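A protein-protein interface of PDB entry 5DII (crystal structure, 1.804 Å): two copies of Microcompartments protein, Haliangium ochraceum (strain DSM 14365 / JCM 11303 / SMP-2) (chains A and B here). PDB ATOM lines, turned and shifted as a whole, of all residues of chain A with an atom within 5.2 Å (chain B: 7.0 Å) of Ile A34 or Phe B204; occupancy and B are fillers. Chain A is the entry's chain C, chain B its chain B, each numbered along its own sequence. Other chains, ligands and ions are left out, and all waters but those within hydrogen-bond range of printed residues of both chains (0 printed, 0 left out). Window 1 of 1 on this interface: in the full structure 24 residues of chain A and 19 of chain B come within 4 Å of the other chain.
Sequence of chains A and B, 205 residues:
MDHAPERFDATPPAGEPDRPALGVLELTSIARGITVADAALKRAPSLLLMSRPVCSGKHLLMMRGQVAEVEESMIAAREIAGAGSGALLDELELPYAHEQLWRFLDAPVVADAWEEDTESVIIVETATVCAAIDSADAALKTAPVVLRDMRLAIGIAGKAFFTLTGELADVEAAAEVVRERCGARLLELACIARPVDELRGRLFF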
ATOM      1  N   ILE A  30       1.143  -0.094   1.287  1.00  0.00           N
ATOM      2  CA  ILE A  30       0.325   0.802   0.491  1.00  0.00           C
ATOM      3  C   ILE A  30      -0.801   0.009  -0.214  1.00  0.00           C
ATOM      4  O   ILE A  30      -1.962   0.432  -0.203  1.00  0.00           O
ATOM      5  CB  ILE A  30       1.216   1.591  -0.499  1.00  0.00           C
ATOM      6  CG1 ILE A  30       2.161   2.521   0.295  1.00  0.00           C
ATOM      7  CG2 ILE A  30       0.383   2.398  -1.482  1.00  0.00           C
ATOM      8  CD1 ILE A  30       3.438   2.834  -0.377  1.00  0.00           C
ATOM      9  N   ALA A  31      -0.476  -1.160  -0.759  1.00  0.00           N
ATOM     10  CA  ALA A  31      -1.471  -1.984  -1.444  1.00  0.00           C
ATOM     11  C   ALA A  31      -2.607  -2.399  -0.505  1.00  0.00           C
ATOM     12  O   ALA A  31      -3.779  -2.255  -0.850  1.00  0.00           O
ATOM     13  CB  ALA A  31      -0.803  -3.228  -2.052  1.00  0.00           C
ATOM     14  N   ARG A  32      -2.259  -2.899   0.675  1.00  0.00           N
ATOM     15  CA  ARG A  32      -3.248  -3.250   1.692  1.00  0.00           C
ATOM     16  C   ARG A  32      -4.096  -2.037   2.087  1.00  0.00           C
ATOM     17  O   ARG A  32      -5.296  -2.155   2.312  1.00  0.00           O
ATOM     18  CB  ARG A  32      -2.558  -3.835   2.924  1.00  0.00           C
ATOM     19  CG  ARG A  32      -3.502  -4.429   3.955  1.00  0.00           C
ATOM     20  CD  ARG A  32      -4.164  -5.702   3.476  1.00  0.00           C
ATOM     21  NE  ARG A  32      -3.203  -6.781   3.283  1.00  0.00           N
ATOM     22  CZ  ARG A  32      -2.796  -7.606   4.245  1.00  0.00           C
ATOM     23  NH1 ARG A  32      -3.263  -7.477   5.482  1.00  0.00           N
ATOM     24  NH2 ARG A  32      -1.908  -8.557   3.974  1.00  0.00           N
ATOM     25  N   GLY A  33      -3.459  -0.882   2.189  1.00  0.00           N
ATOM     26  CA  GLY A  33      -4.131   0.367   2.513  1.00  0.00           C
ATOM     27  C   GLY A  33      -5.274   0.724   1.581  1.00  0.00           C
ATOM     28  O   GLY A  33      -6.308   1.258   2.014  1.00  0.00           O
ATOM     29  N   ILE A  34      -5.071   0.499   0.287  1.00  0.00           N
ATOM     30  CA  ILE A  34      -6.114   0.775  -0.686  1.00  0.00           C
ATOM     31  C   ILE A  34      -7.290  -0.188  -0.443  1.00  0.00           C
ATOM     32  O   ILE A  34      -8.436   0.239  -0.378  1.00  0.00           O
ATOM     33  CB  ILE A  34      -5.558   0.671  -2.126  1.00  0.00           C
ATOM     34  CG1 ILE A  34      -4.427   1.703  -2.304  1.00  0.00           C
ATOM     35  CG2 ILE A  34      -6.668   0.860  -3.164  1.00  0.00           C
ATOM     36  CD1 ILE A  34      -4.824   3.153  -2.071  1.00  0.00           C
ATOM     37  N   THR A  35      -7.003  -1.460  -0.192  1.00  0.00           N
ATOM     38  CA  THR A  35      -8.068  -2.433   0.029  1.00  0.00           C
ATOM     39  C   THR A  35      -8.814  -2.141   1.328  1.00  0.00           C
ATOM     40  O   THR A  35     -10.021  -2.341   1.399  1.00  0.00           O
ATOM     41  CB  THR A  35      -7.542  -3.879   0.089  1.00  0.00           C
ATOM     42  OG1 THR A  35      -6.723  -4.053   1.246  1.00  0.00           O
ATOM     43  CG2 THR A  35      -6.731  -4.192  -1.109  1.00  0.00           C
ATOM     44  N   VAL A  36      -8.081  -1.684   2.339  1.00  0.00           N
ATOM     45  CA  VAL A  36      -8.663  -1.273   3.608  1.00  0.00           C
ATOM     46  C   VAL A  36      -9.612  -0.096   3.396  1.00  0.00           C
ATOM     47  O   VAL A  36     -10.754  -0.124   3.886  1.00  0.00           O
ATOM     48  CB  VAL A  36      -7.557  -0.906   4.650  1.00  0.00           C
ATOM     49  CG1 VAL A  36      -8.124  -0.134   5.830  1.00  0.00           C
ATOM     50  CG2 VAL A  36      -6.855  -2.160   5.135  1.00  0.00           C
ATOM     51  N   ALA A  37      -9.171   0.906   2.643  1.00  0.00           N
ATOM     52  CA  ALA A  37     -10.011   2.053   2.328  1.00  0.00           C
ATOM     53  C   ALA A  37     -11.310   1.622   1.636  1.00  0.00           C
ATOM     54  O   ALA A  37     -12.396   2.069   2.002  1.00  0.00           O
ATOM     55  CB  ALA A  37      -9.260   3.036   1.446  1.00  0.00           C
ATOM     56  N   ASP A  38     -11.171   0.754   0.641  1.00  0.00           N
ATOM     57  CA  ASP A  38     -12.298   0.232  -0.128  1.00  0.00           C
ATOM     58  C   ASP A  38     -13.300  -0.485   0.781  1.00  0.00           C
ATOM     59  O   ASP A  38     -14.494  -0.206   0.743  1.00  0.00           O
ATOM     60  CB  ASP A  38     -11.769  -0.697  -1.225  1.00  0.00           C
ATOM     61  CG  ASP A  38     -12.868  -1.290  -2.066  1.00  0.00           C
ATOM     62  OD1 ASP A  38     -13.522  -0.547  -2.831  1.00  0.00           O
ATOM     63  OD2 ASP A  38     -13.036  -2.519  -1.983  1.00  0.00           O
ATOM     64  N   ALA A  39     -12.800  -1.382   1.620  1.00  0.00           N
ATOM     65  CA  ALA A  39     -13.632  -2.078   2.588  1.00  0.00           C
ATOM     66  C   ALA A  39     -14.335  -1.139   3.577  1.00  0.00           C
ATOM     67  O   ALA A  39     -15.507  -1.360   3.924  1.00  0.00           O
ATOM     68  CB  ALA A  39     -12.797  -3.085   3.353  1.00  0.00           C
ATOM     69  N   SER A  51      -5.749   9.229   1.476  1.00  0.00           N
ATOM     70  CA  SER A  51      -5.215   7.907   1.206  1.00  0.00           C
ATOM     71  C   SER A  51      -3.809   8.126   0.648  1.00  0.00           C
ATOM     72  O   SER A  51      -3.628   8.408  -0.544  1.00  0.00           O
ATOM     73  CB  SER A  51      -6.119   7.141   0.226  1.00  0.00           C
ATOM     74  OG  SER A  51      -5.591   5.862  -0.065  1.00  0.00           O
ATOM     75  N   PRO A  53       0.503   7.355   0.661  1.00  0.00           N
ATOM     76  CA  PRO A  53       1.785   6.805   1.070  1.00  0.00           C
ATOM     77  C   PRO A  53       2.578   7.920   1.746  1.00  0.00           C
ATOM     78  O   PRO A  53       2.566   9.050   1.264  1.00  0.00           O
ATOM     79  CB  PRO A  53       2.438   6.377  -0.248  1.00  0.00           C
ATOM     80  CG  PRO A  53       1.349   6.404  -1.251  1.00  0.00           C
ATOM     81  CD  PRO A  53       0.403   7.446  -0.805  1.00  0.00           C
ATOM     82  N   HIS A  59       1.269   3.614   4.807  1.00  0.00           N
ATOM     83  CA  HIS A  59       0.139   4.232   4.136  1.00  0.00           C
ATOM     84  C   HIS A  59      -0.774   4.830   5.188  1.00  0.00           C
ATOM     85  O   HIS A  59      -1.038   4.194   6.193  1.00  0.00           O
ATOM     86  CB  HIS A  59      -0.604   3.207   3.276  1.00  0.00           C
ATOM     87  CG  HIS A  59      -1.588   3.823   2.332  1.00  0.00           C
ATOM     88  ND1 HIS A  59      -1.203   4.404   1.144  1.00  0.00           N
ATOM     89  CD2 HIS A  59      -2.934   3.959   2.402  1.00  0.00           C
ATOM     90  CE1 HIS A  59      -2.267   4.888   0.529  1.00  0.00           C
ATOM     91  NE2 HIS A  59      -3.331   4.625   1.271  1.00  0.00           N
ATOM     92  N   VAL B 109       3.647   9.522 -10.433  1.00  0.00           N
ATOM     93  CA  VAL B 109       2.445   9.874 -11.180  1.00  0.00           C
ATOM     94  C   VAL B 109       1.250   9.375 -10.404  1.00  0.00           C
ATOM     95  O   VAL B 109       1.226   8.218 -10.002  1.00  0.00           O
ATOM     96  CB  VAL B 109       2.449   9.254 -12.603  1.00  0.00           C
ATOM     97  CG1 VAL B 109       1.101   9.463 -13.313  1.00  0.00           C
ATOM     98  CG2 VAL B 109       3.626   9.800 -13.430  1.00  0.00           C
ATOM     99  N   VAL B 110       0.275  10.252 -10.176  1.00  0.00           N
ATOM    100  CA  VAL B 110      -0.992   9.844  -9.578  1.00  0.00           C
ATOM    101  C   VAL B 110      -2.087  10.170 -10.585  1.00  0.00           C
ATOM    102  O   VAL B 110      -2.163  11.286 -11.093  1.00  0.00           O
ATOM    103  CB  VAL B 110      -1.252  10.521  -8.209  1.00  0.00           C
ATOM    104  CG1 VAL B 110      -1.245  12.039  -8.319  1.00  0.00           C
ATOM    105  CG2 VAL B 110      -2.570  10.024  -7.605  1.00  0.00           C
ATOM    106  N   ALA B 111      -2.914   9.174 -10.893  1.00  0.00           N
ATOM    107  CA  ALA B 111      -4.003   9.337 -11.851  1.00  0.00           C
ATOM    108  C   ALA B 111      -5.153  10.147 -11.269  1.00  0.00           C
ATOM    109  O   ALA B 111      -5.476  10.022 -10.088  1.00  0.00           O
ATOM    110  CB  ALA B 111      -4.512   7.974 -12.309  1.00  0.00           C
ATOM    111  N   ASP B 112      -5.749  10.985 -12.114  1.00  0.00           N
ATOM    112  CA  ASP B 112      -6.919  11.782 -11.752  1.00  0.00           C
ATOM    113  C   ASP B 112      -8.202  11.030 -12.085  1.00  0.00           C
ATOM    114  O   ASP B 112      -9.215  11.182 -11.404  1.00  0.00           O
ATOM    115  CB  ASP B 112      -6.915  13.126 -12.492  1.00  0.00           C
ATOM    116  CG  ASP B 112      -5.907  14.105 -11.932  1.00  0.00           C
ATOM    117  OD1 ASP B 112      -5.551  13.993 -10.739  1.00  0.00           O
ATOM    118  OD2 ASP B 112      -5.469  14.993 -12.692  1.00  0.00           O
ATOM    119  N   VAL B 121      -8.818  -2.922 -10.658  1.00  0.00           N
ATOM    120  CA  VAL B 121      -7.477  -2.405 -10.405  1.00  0.00           C
ATOM    121  C   VAL B 121      -6.638  -3.422  -9.625  1.00  0.00           C
ATOM    122  O   VAL B 121      -7.150  -4.118  -8.743  1.00  0.00           O
ATOM    123  CB  VAL B 121      -7.533  -1.057  -9.622  1.00  0.00           C
ATOM    124  CG1 VAL B 121      -8.150  -1.239  -8.255  1.00  0.00           C
ATOM    125  CG2 VAL B 121      -6.135  -0.432  -9.504  1.00  0.00           C
ATOM    126  N   ILE B 123      -2.930  -3.274  -7.351  1.00  0.00           N
ATOM    127  CA  ILE B 123      -1.923  -2.430  -6.749  1.00  0.00           C
ATOM    128  C   ILE B 123      -0.753  -3.308  -6.428  1.00  0.00           C
ATOM    129  O   ILE B 123      -0.888  -4.264  -5.681  1.00  0.00           O
ATOM    130  CB  ILE B 123      -2.438  -1.729  -5.464  1.00  0.00           C
ATOM    131  CG1 ILE B 123      -3.704  -0.928  -5.761  1.00  0.00           C
ATOM    132  CG2 ILE B 123      -1.406  -0.799  -4.902  1.00  0.00           C
ATOM    133  CD1 ILE B 123      -4.973  -1.611  -5.347  1.00  0.00           C
ATOM    134  N   ASP B 149      -0.876   4.642 -11.807  1.00  0.00           N
ATOM    135  CA  ASP B 149      -0.092   5.276 -10.756  1.00  0.00           C
ATOM    136  C   ASP B 149       1.279   4.615 -10.718  1.00  0.00           C
ATOM    137  O   ASP B 149       1.421   3.435 -11.050  1.00  0.00           O
ATOM    138  CB  ASP B 149      -0.750   5.146  -9.376  1.00  0.00           C
ATOM    139  CG  ASP B 149      -2.199   5.623  -9.345  1.00  0.00           C
ATOM    140  OD1 ASP B 149      -2.431   6.848  -9.243  1.00  0.00           O
ATOM    141  OD2 ASP B 149      -3.105   4.768  -9.387  1.00  0.00           O
ATOM    142  N   MET B 150       2.299   5.374 -10.342  1.00  0.00           N
ATOM    143  CA  MET B 150       3.576   4.757 -10.046  1.00  0.00           C
ATOM    144  C   MET B 150       4.384   5.688  -9.123  1.00  0.00           C
ATOM    145  O   MET B 150       4.283   6.917  -9.200  1.00  0.00           O
ATOM    146  CB  MET B 150       4.345   4.435 -11.329  1.00  0.00           C
ATOM    147  CG  MET B 150       5.641   3.722 -11.066  1.00  0.00           C
ATOM    148  SD  MET B 150       6.512   3.185 -12.538  1.00  0.00           S
ATOM    149  CE  MET B 150       5.716   1.613 -12.871  1.00  0.00           C
ATOM    150  N   PHE B 161       5.755   1.233  -6.008  1.00  0.00           N
ATOM    151  CA  PHE B 161       4.476   0.639  -6.305  1.00  0.00           C
ATOM    152  C   PHE B 161       3.925   1.197  -7.588  1.00  0.00           C
ATOM    153  O   PHE B 161       4.343   2.245  -8.051  1.00  0.00           O
ATOM    154  CB  PHE B 161       3.464   0.844  -5.163  1.00  0.00           C
ATOM    155  CG  PHE B 161       3.011   2.267  -4.983  1.00  0.00           C
ATOM    156  CD1 PHE B 161       1.991   2.792  -5.770  1.00  0.00           C
ATOM    157  CD2 PHE B 161       3.578   3.075  -4.013  1.00  0.00           C
ATOM    158  CE1 PHE B 161       1.565   4.101  -5.592  1.00  0.00           C
ATOM    159  CE2 PHE B 161       3.148   4.389  -3.831  1.00  0.00           C
ATOM    160  CZ  PHE B 161       2.160   4.901  -4.629  1.00  0.00           C
ATOM    161  N   PHE B 162       2.969   0.472  -8.164  1.00  0.00           N
ATOM    162  CA  PHE B 162       2.256   0.963  -9.328  1.00  0.00           C
ATOM    163  C   PHE B 162       0.870   0.309  -9.359  1.00  0.00           C
ATOM    164  O   PHE B 162       0.610  -0.665  -8.649  1.00  0.00           O
ATOM    165  CB  PHE B 162       3.036   0.677 -10.624  1.00  0.00           C
ATOM    166  CG  PHE B 162       3.219  -0.783 -10.917  1.00  0.00           C
ATOM    167  CD1 PHE B 162       2.275  -1.485 -11.657  1.00  0.00           C
ATOM    168  CD2 PHE B 162       4.325  -1.459 -10.432  1.00  0.00           C
ATOM    169  CE1 PHE B 162       2.463  -2.829 -11.945  1.00  0.00           C
ATOM    170  CE2 PHE B 162       4.524  -2.787 -10.715  1.00  0.00           C
ATOM    171  CZ  PHE B 162       3.587  -3.486 -11.464  1.00  0.00           C
ATOM    172  N   THR B 163      -0.019   0.900 -10.140  1.00  0.00           N
ATOM    173  CA  THR B 163      -1.349   0.361 -10.334  1.00  0.00           C
ATOM    174  C   THR B 163      -1.626   0.103 -11.794  1.00  0.00           C
ATOM    175  O   THR B 163      -1.172   0.839 -12.666  1.00  0.00           O
ATOM    176  CB  THR B 163      -2.424   1.308  -9.769  1.00  0.00           C
ATOM    177  OG1 THR B 163      -2.359   2.565 -10.451  1.00  0.00           O
ATOM    178  CG2 THR B 163      -2.216   1.522  -8.290  1.00  0.00           C
ATOM    179  N   ALA B 190      -2.511  -6.284  -4.377  1.00  0.00           N
ATOM    180  CA  ALA B 190      -3.916  -6.214  -4.015  1.00  0.00           C
ATOM    181  C   ALA B 190      -4.735  -6.116  -5.289  1.00  0.00           C
ATOM    182  O   ALA B 190      -4.338  -5.458  -6.248  1.00  0.00           O
ATOM    183  CB  ALA B 190      -4.184  -5.037  -3.118  1.00  0.00           C
ATOM    184  N   ILE B 192      -8.693  -5.265  -6.577  1.00  0.00           N
ATOM    185  CA  ILE B 192     -10.025  -4.791  -6.247  1.00  0.00           C
ATOM    186  C   ILE B 192     -10.905  -4.855  -7.492  1.00  0.00           C
ATOM    187  O   ILE B 192     -10.722  -4.070  -8.433  1.00  0.00           O
ATOM    188  CB  ILE B 192      -9.973  -3.356  -5.692  1.00  0.00           C
ATOM    189  CG1 ILE B 192      -9.087  -3.289  -4.447  1.00  0.00           C
ATOM    190  CG2 ILE B 192     -11.362  -2.860  -5.327  1.00  0.00           C
ATOM    191  CD1 ILE B 192      -8.820  -1.887  -3.978  1.00  0.00           C
ATOM    192  N   PRO B 195     -13.842  -1.188  -7.225  1.00  0.00           N
ATOM    193  CA  PRO B 195     -13.584  -0.133  -6.221  1.00  0.00           C
ATOM    194  C   PRO B 195     -14.830   0.698  -5.877  1.00  0.00           C
ATOM    195  O   PRO B 195     -15.594   0.963  -6.792  1.00  0.00           O
ATOM    196  CB  PRO B 195     -12.537   0.755  -6.914  1.00  0.00           C
ATOM    197  CG  PRO B 195     -11.906  -0.100  -7.984  1.00  0.00           C
ATOM    198  CD  PRO B 195     -12.963  -1.096  -8.408  1.00  0.00           C
ATOM    199  N   LEU B 199     -13.464   5.931  -4.519  1.00  0.00           N
ATOM    200  CA  LEU B 199     -12.069   5.635  -4.838  1.00  0.00           C
ATOM    201  C   LEU B 199     -11.770   5.548  -6.327  1.00  0.00           C
ATOM    202  O   LEU B 199     -10.619   5.686  -6.741  1.00  0.00           O
ATOM    203  CB  LEU B 199     -11.647   4.323  -4.194  1.00  0.00           C
ATOM    204  CG  LEU B 199     -11.260   4.279  -2.725  1.00  0.00           C
ATOM    205  CD1 LEU B 199     -10.704   2.914  -2.380  1.00  0.00           C
ATOM    206  CD2 LEU B 199     -10.317   5.425  -2.315  1.00  0.00           C
ATOM    207  N   GLY B 201     -10.954   6.005 -10.017  1.00  0.00           N
ATOM    208  CA  GLY B 201     -10.206   7.044 -10.690  1.00  0.00           C
ATOM    209  C   GLY B 201      -9.058   7.548  -9.836  1.00  0.00           C
ATOM    210  O   GLY B 201      -7.911   7.546 -10.289  1.00  0.00           O
ATOM    211  N   ARG B 202      -9.366   8.033  -8.635  1.00  0.00           N
ATOM    212  CA  ARG B 202      -8.338   8.527  -7.730  1.00  0.00           C
ATOM    213  C   ARG B 202      -8.147   7.665  -6.465  1.00  0.00           C
ATOM    214  O   ARG B 202      -8.918   7.768  -5.516  1.00  0.00           O
ATOM    215  CB  ARG B 202      -8.706   9.948  -7.337  1.00  0.00           C
ATOM    216  CG  ARG B 202      -7.644  10.712  -6.579  1.00  0.00           C
ATOM    217  CD  ARG B 202      -8.115  12.140  -6.434  1.00  0.00           C
ATOM    218  NE  ARG B 202      -8.196  12.821  -7.722  1.00  0.00           N
ATOM    219  CZ  ARG B 202      -8.549  14.092  -7.874  1.00  0.00           C
ATOM    220  NH1 ARG B 202      -8.610  14.620  -9.088  1.00  0.00           N
ATOM    221  NH2 ARG B 202      -8.848  14.837  -6.814  1.00  0.00           N
ATOM    222  N   LEU B 203      -7.013   6.982  -6.370  1.00  0.00           N
ATOM    223  CA  LEU B 203      -6.747   6.068  -5.256  1.00  0.00           C
ATOM    224  C   LEU B 203      -5.871   6.722  -4.188  1.00  0.00           C
ATOM    225  O   LEU B 203      -5.797   6.265  -3.051  1.00  0.00           O
ATOM    226  CB  LEU B 203      -6.031   4.822  -5.753  1.00  0.00           C
ATOM    227  CG  LEU B 203      -6.774   3.856  -6.688  1.00  0.00           C
ATOM    228  CD1 LEU B 203      -5.882   2.671  -7.042  1.00  0.00           C
ATOM    229  CD2 LEU B 203      -8.102   3.417  -6.071  1.00  0.00           C
ATOM    230  N   PHE B 204      -5.153   7.744  -4.610  1.00  0.00           N
ATOM    231  CA  PHE B 204      -4.210   8.449  -3.749  1.00  0.00           C
ATOM    232  C   PHE B 204      -4.581   9.919  -3.781  1.00  0.00           C
ATOM    233  O   PHE B 204      -4.714  10.511  -4.860  1.00  0.00           O
ATOM    234  CB  PHE B 204      -2.786   8.207  -4.201  1.00  0.00           C
ATOM    235  CG  PHE B 204      -2.446   6.757  -4.360  1.00  0.00           C
ATOM    236  CD1 PHE B 204      -2.113   5.989  -3.257  1.00  0.00           C
ATOM    237  CD2 PHE B 204      -2.447   6.162  -5.613  1.00  0.00           C
ATOM    238  CE1 PHE B 204      -1.798   4.648  -3.399  1.00  0.00           C
ATOM    239  CE2 PHE B 204      -2.133   4.825  -5.762  1.00  0.00           C
ATOM    240  CZ  PHE B 204      -1.803   4.065  -4.651  1.00  0.00           C
ATOM    241  N   PHE B 205      -4.796  10.489  -2.596  1.00  0.00           N
ATOM    242  CA  PHE B 205      -5.213  11.879  -2.464  1.00  0.00           C
ATOM    243  C   PHE B 205      -5.092  12.380  -1.031  1.00  0.00           C
ATOM    244  O   PHE B 205      -4.692  11.659  -0.106  1.00  0.00           O
ATOM    245  CB  PHE B 205      -6.668  12.024  -2.924  1.00  0.00           C
ATOM    246  CG  PHE B 205      -7.642  11.223  -2.093  1.00  0.00           C
ATOM    247  CD1 PHE B 205      -8.240  11.778  -0.974  1.00  0.00           C
ATOM    248  CD2 PHE B 205      -7.954   9.912  -2.427  1.00  0.00           C
ATOM    249  CE1 PHE B 205      -9.128  11.045  -0.205  1.00  0.00           C
ATOM    250  CE2 PHE B 205      -8.840   9.184  -1.661  1.00  0.00           C
ATOM    251  CZ  PHE B 205      -9.425   9.758  -0.542  1.00  0.00           C
ATOM    252  OXT PHE B 205      -5.454  13.525  -0.761  1.00  0.00           O
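O of Leu B203 sits at hydrogen-bond distance from OG of Ser A51, at 3.0 Å.
The backbone NH (N) of Ser A51 is in hydrogen-bond range of the chain-end carboxylate (O) of Phe B205, 3.1 Å away.
O of Val B121 lies within hydrogen-bond range of N of Ile B192, at 2.9 Å.
The backbone NH (N) of Ile B123 sits at hydrogen-bond distance from the backbone carbonyl oxygen (O) of Ala B190.
The side-chain hydroxyl of Thr A35 is in hydrogen-bond range of the backbone carbonyl oxygen of Arg A32.
A ring nitrogen (NE2) of His A59 is in hydrogen-bond range of the side-chain hydroxyl (OG) of Ser A51 (2.9 Å).
Among the printed residues, merely in contact across the chains: Ile A30 with Phe B161, Ile A30 with Phe B204, Ala A31 with Ile B123, Ala A31 with Ala B190, Ile A34 with Ile B123, Ile A34 with Ile B192, Ile A34 with Leu B203, Ile A34 with Phe B204, Thr A35 with Ala B190, Asp A38 with Ile B192, Asp A38 with Pro B195, Asp A38 with Leu B199, Ser A51 with Phe B204, Pro A53 with Phe B161, Pro A53 with Phe B204 and His A59 with Phe B204.
Ile A34 touches four residues of chain B.
Of chain A, only Ile A30 (3.7 Å), Ile A34 (3.6 Å), Ser A51 (3.3 Å), Pro A53 (3.8 Å) and His A59 (3.9 Å) come within 4 Å of Phe B204.
No residue of chain B comes within 4 Å of Gly A33.
Printed residues of chain A within 4 Å of Ala B190: Ala A31 (3.6 Å) and Thr A35 (3.4 Å).
Of the printed residues of chain A, Phe B205 touches Ser A51 (3.1 Å).
Of the printed residues of chain A, Leu B203 touches Ile A34 and Ser A51.
Of the printed residues of chain A, Ile B192 touches Ile A34 and Asp A38.
The nearest residue of chain B that does not touch Ile A34 is Leu B199 (4.04 Å).
The nearest printed residue of chain A that does not touch Phe B204 is Ala A31 (6.5 Å).
Printed residues of chain A that touch a printed residue of chain B: Ile A30, Ala A31, Ile A34, Thr A35, Asp A38, Ser A51, Pro A53 and His A59.
Along chain A the printed residues that touch a printed residue of chain B span positions 30 to 59.
Along chain B the printed residues that touch a printed residue of chain A span positions 123 to 205.
Among the printed residues, no Asp or Glu carboxylate lies within 4 Å of a Lys or Arg side-chain nitrogen of the other chain.
No position is printed for both chains.
Of the 18 pairs that touch across the chains among the printed residues, none has its exchanged pair printed and touching as well.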
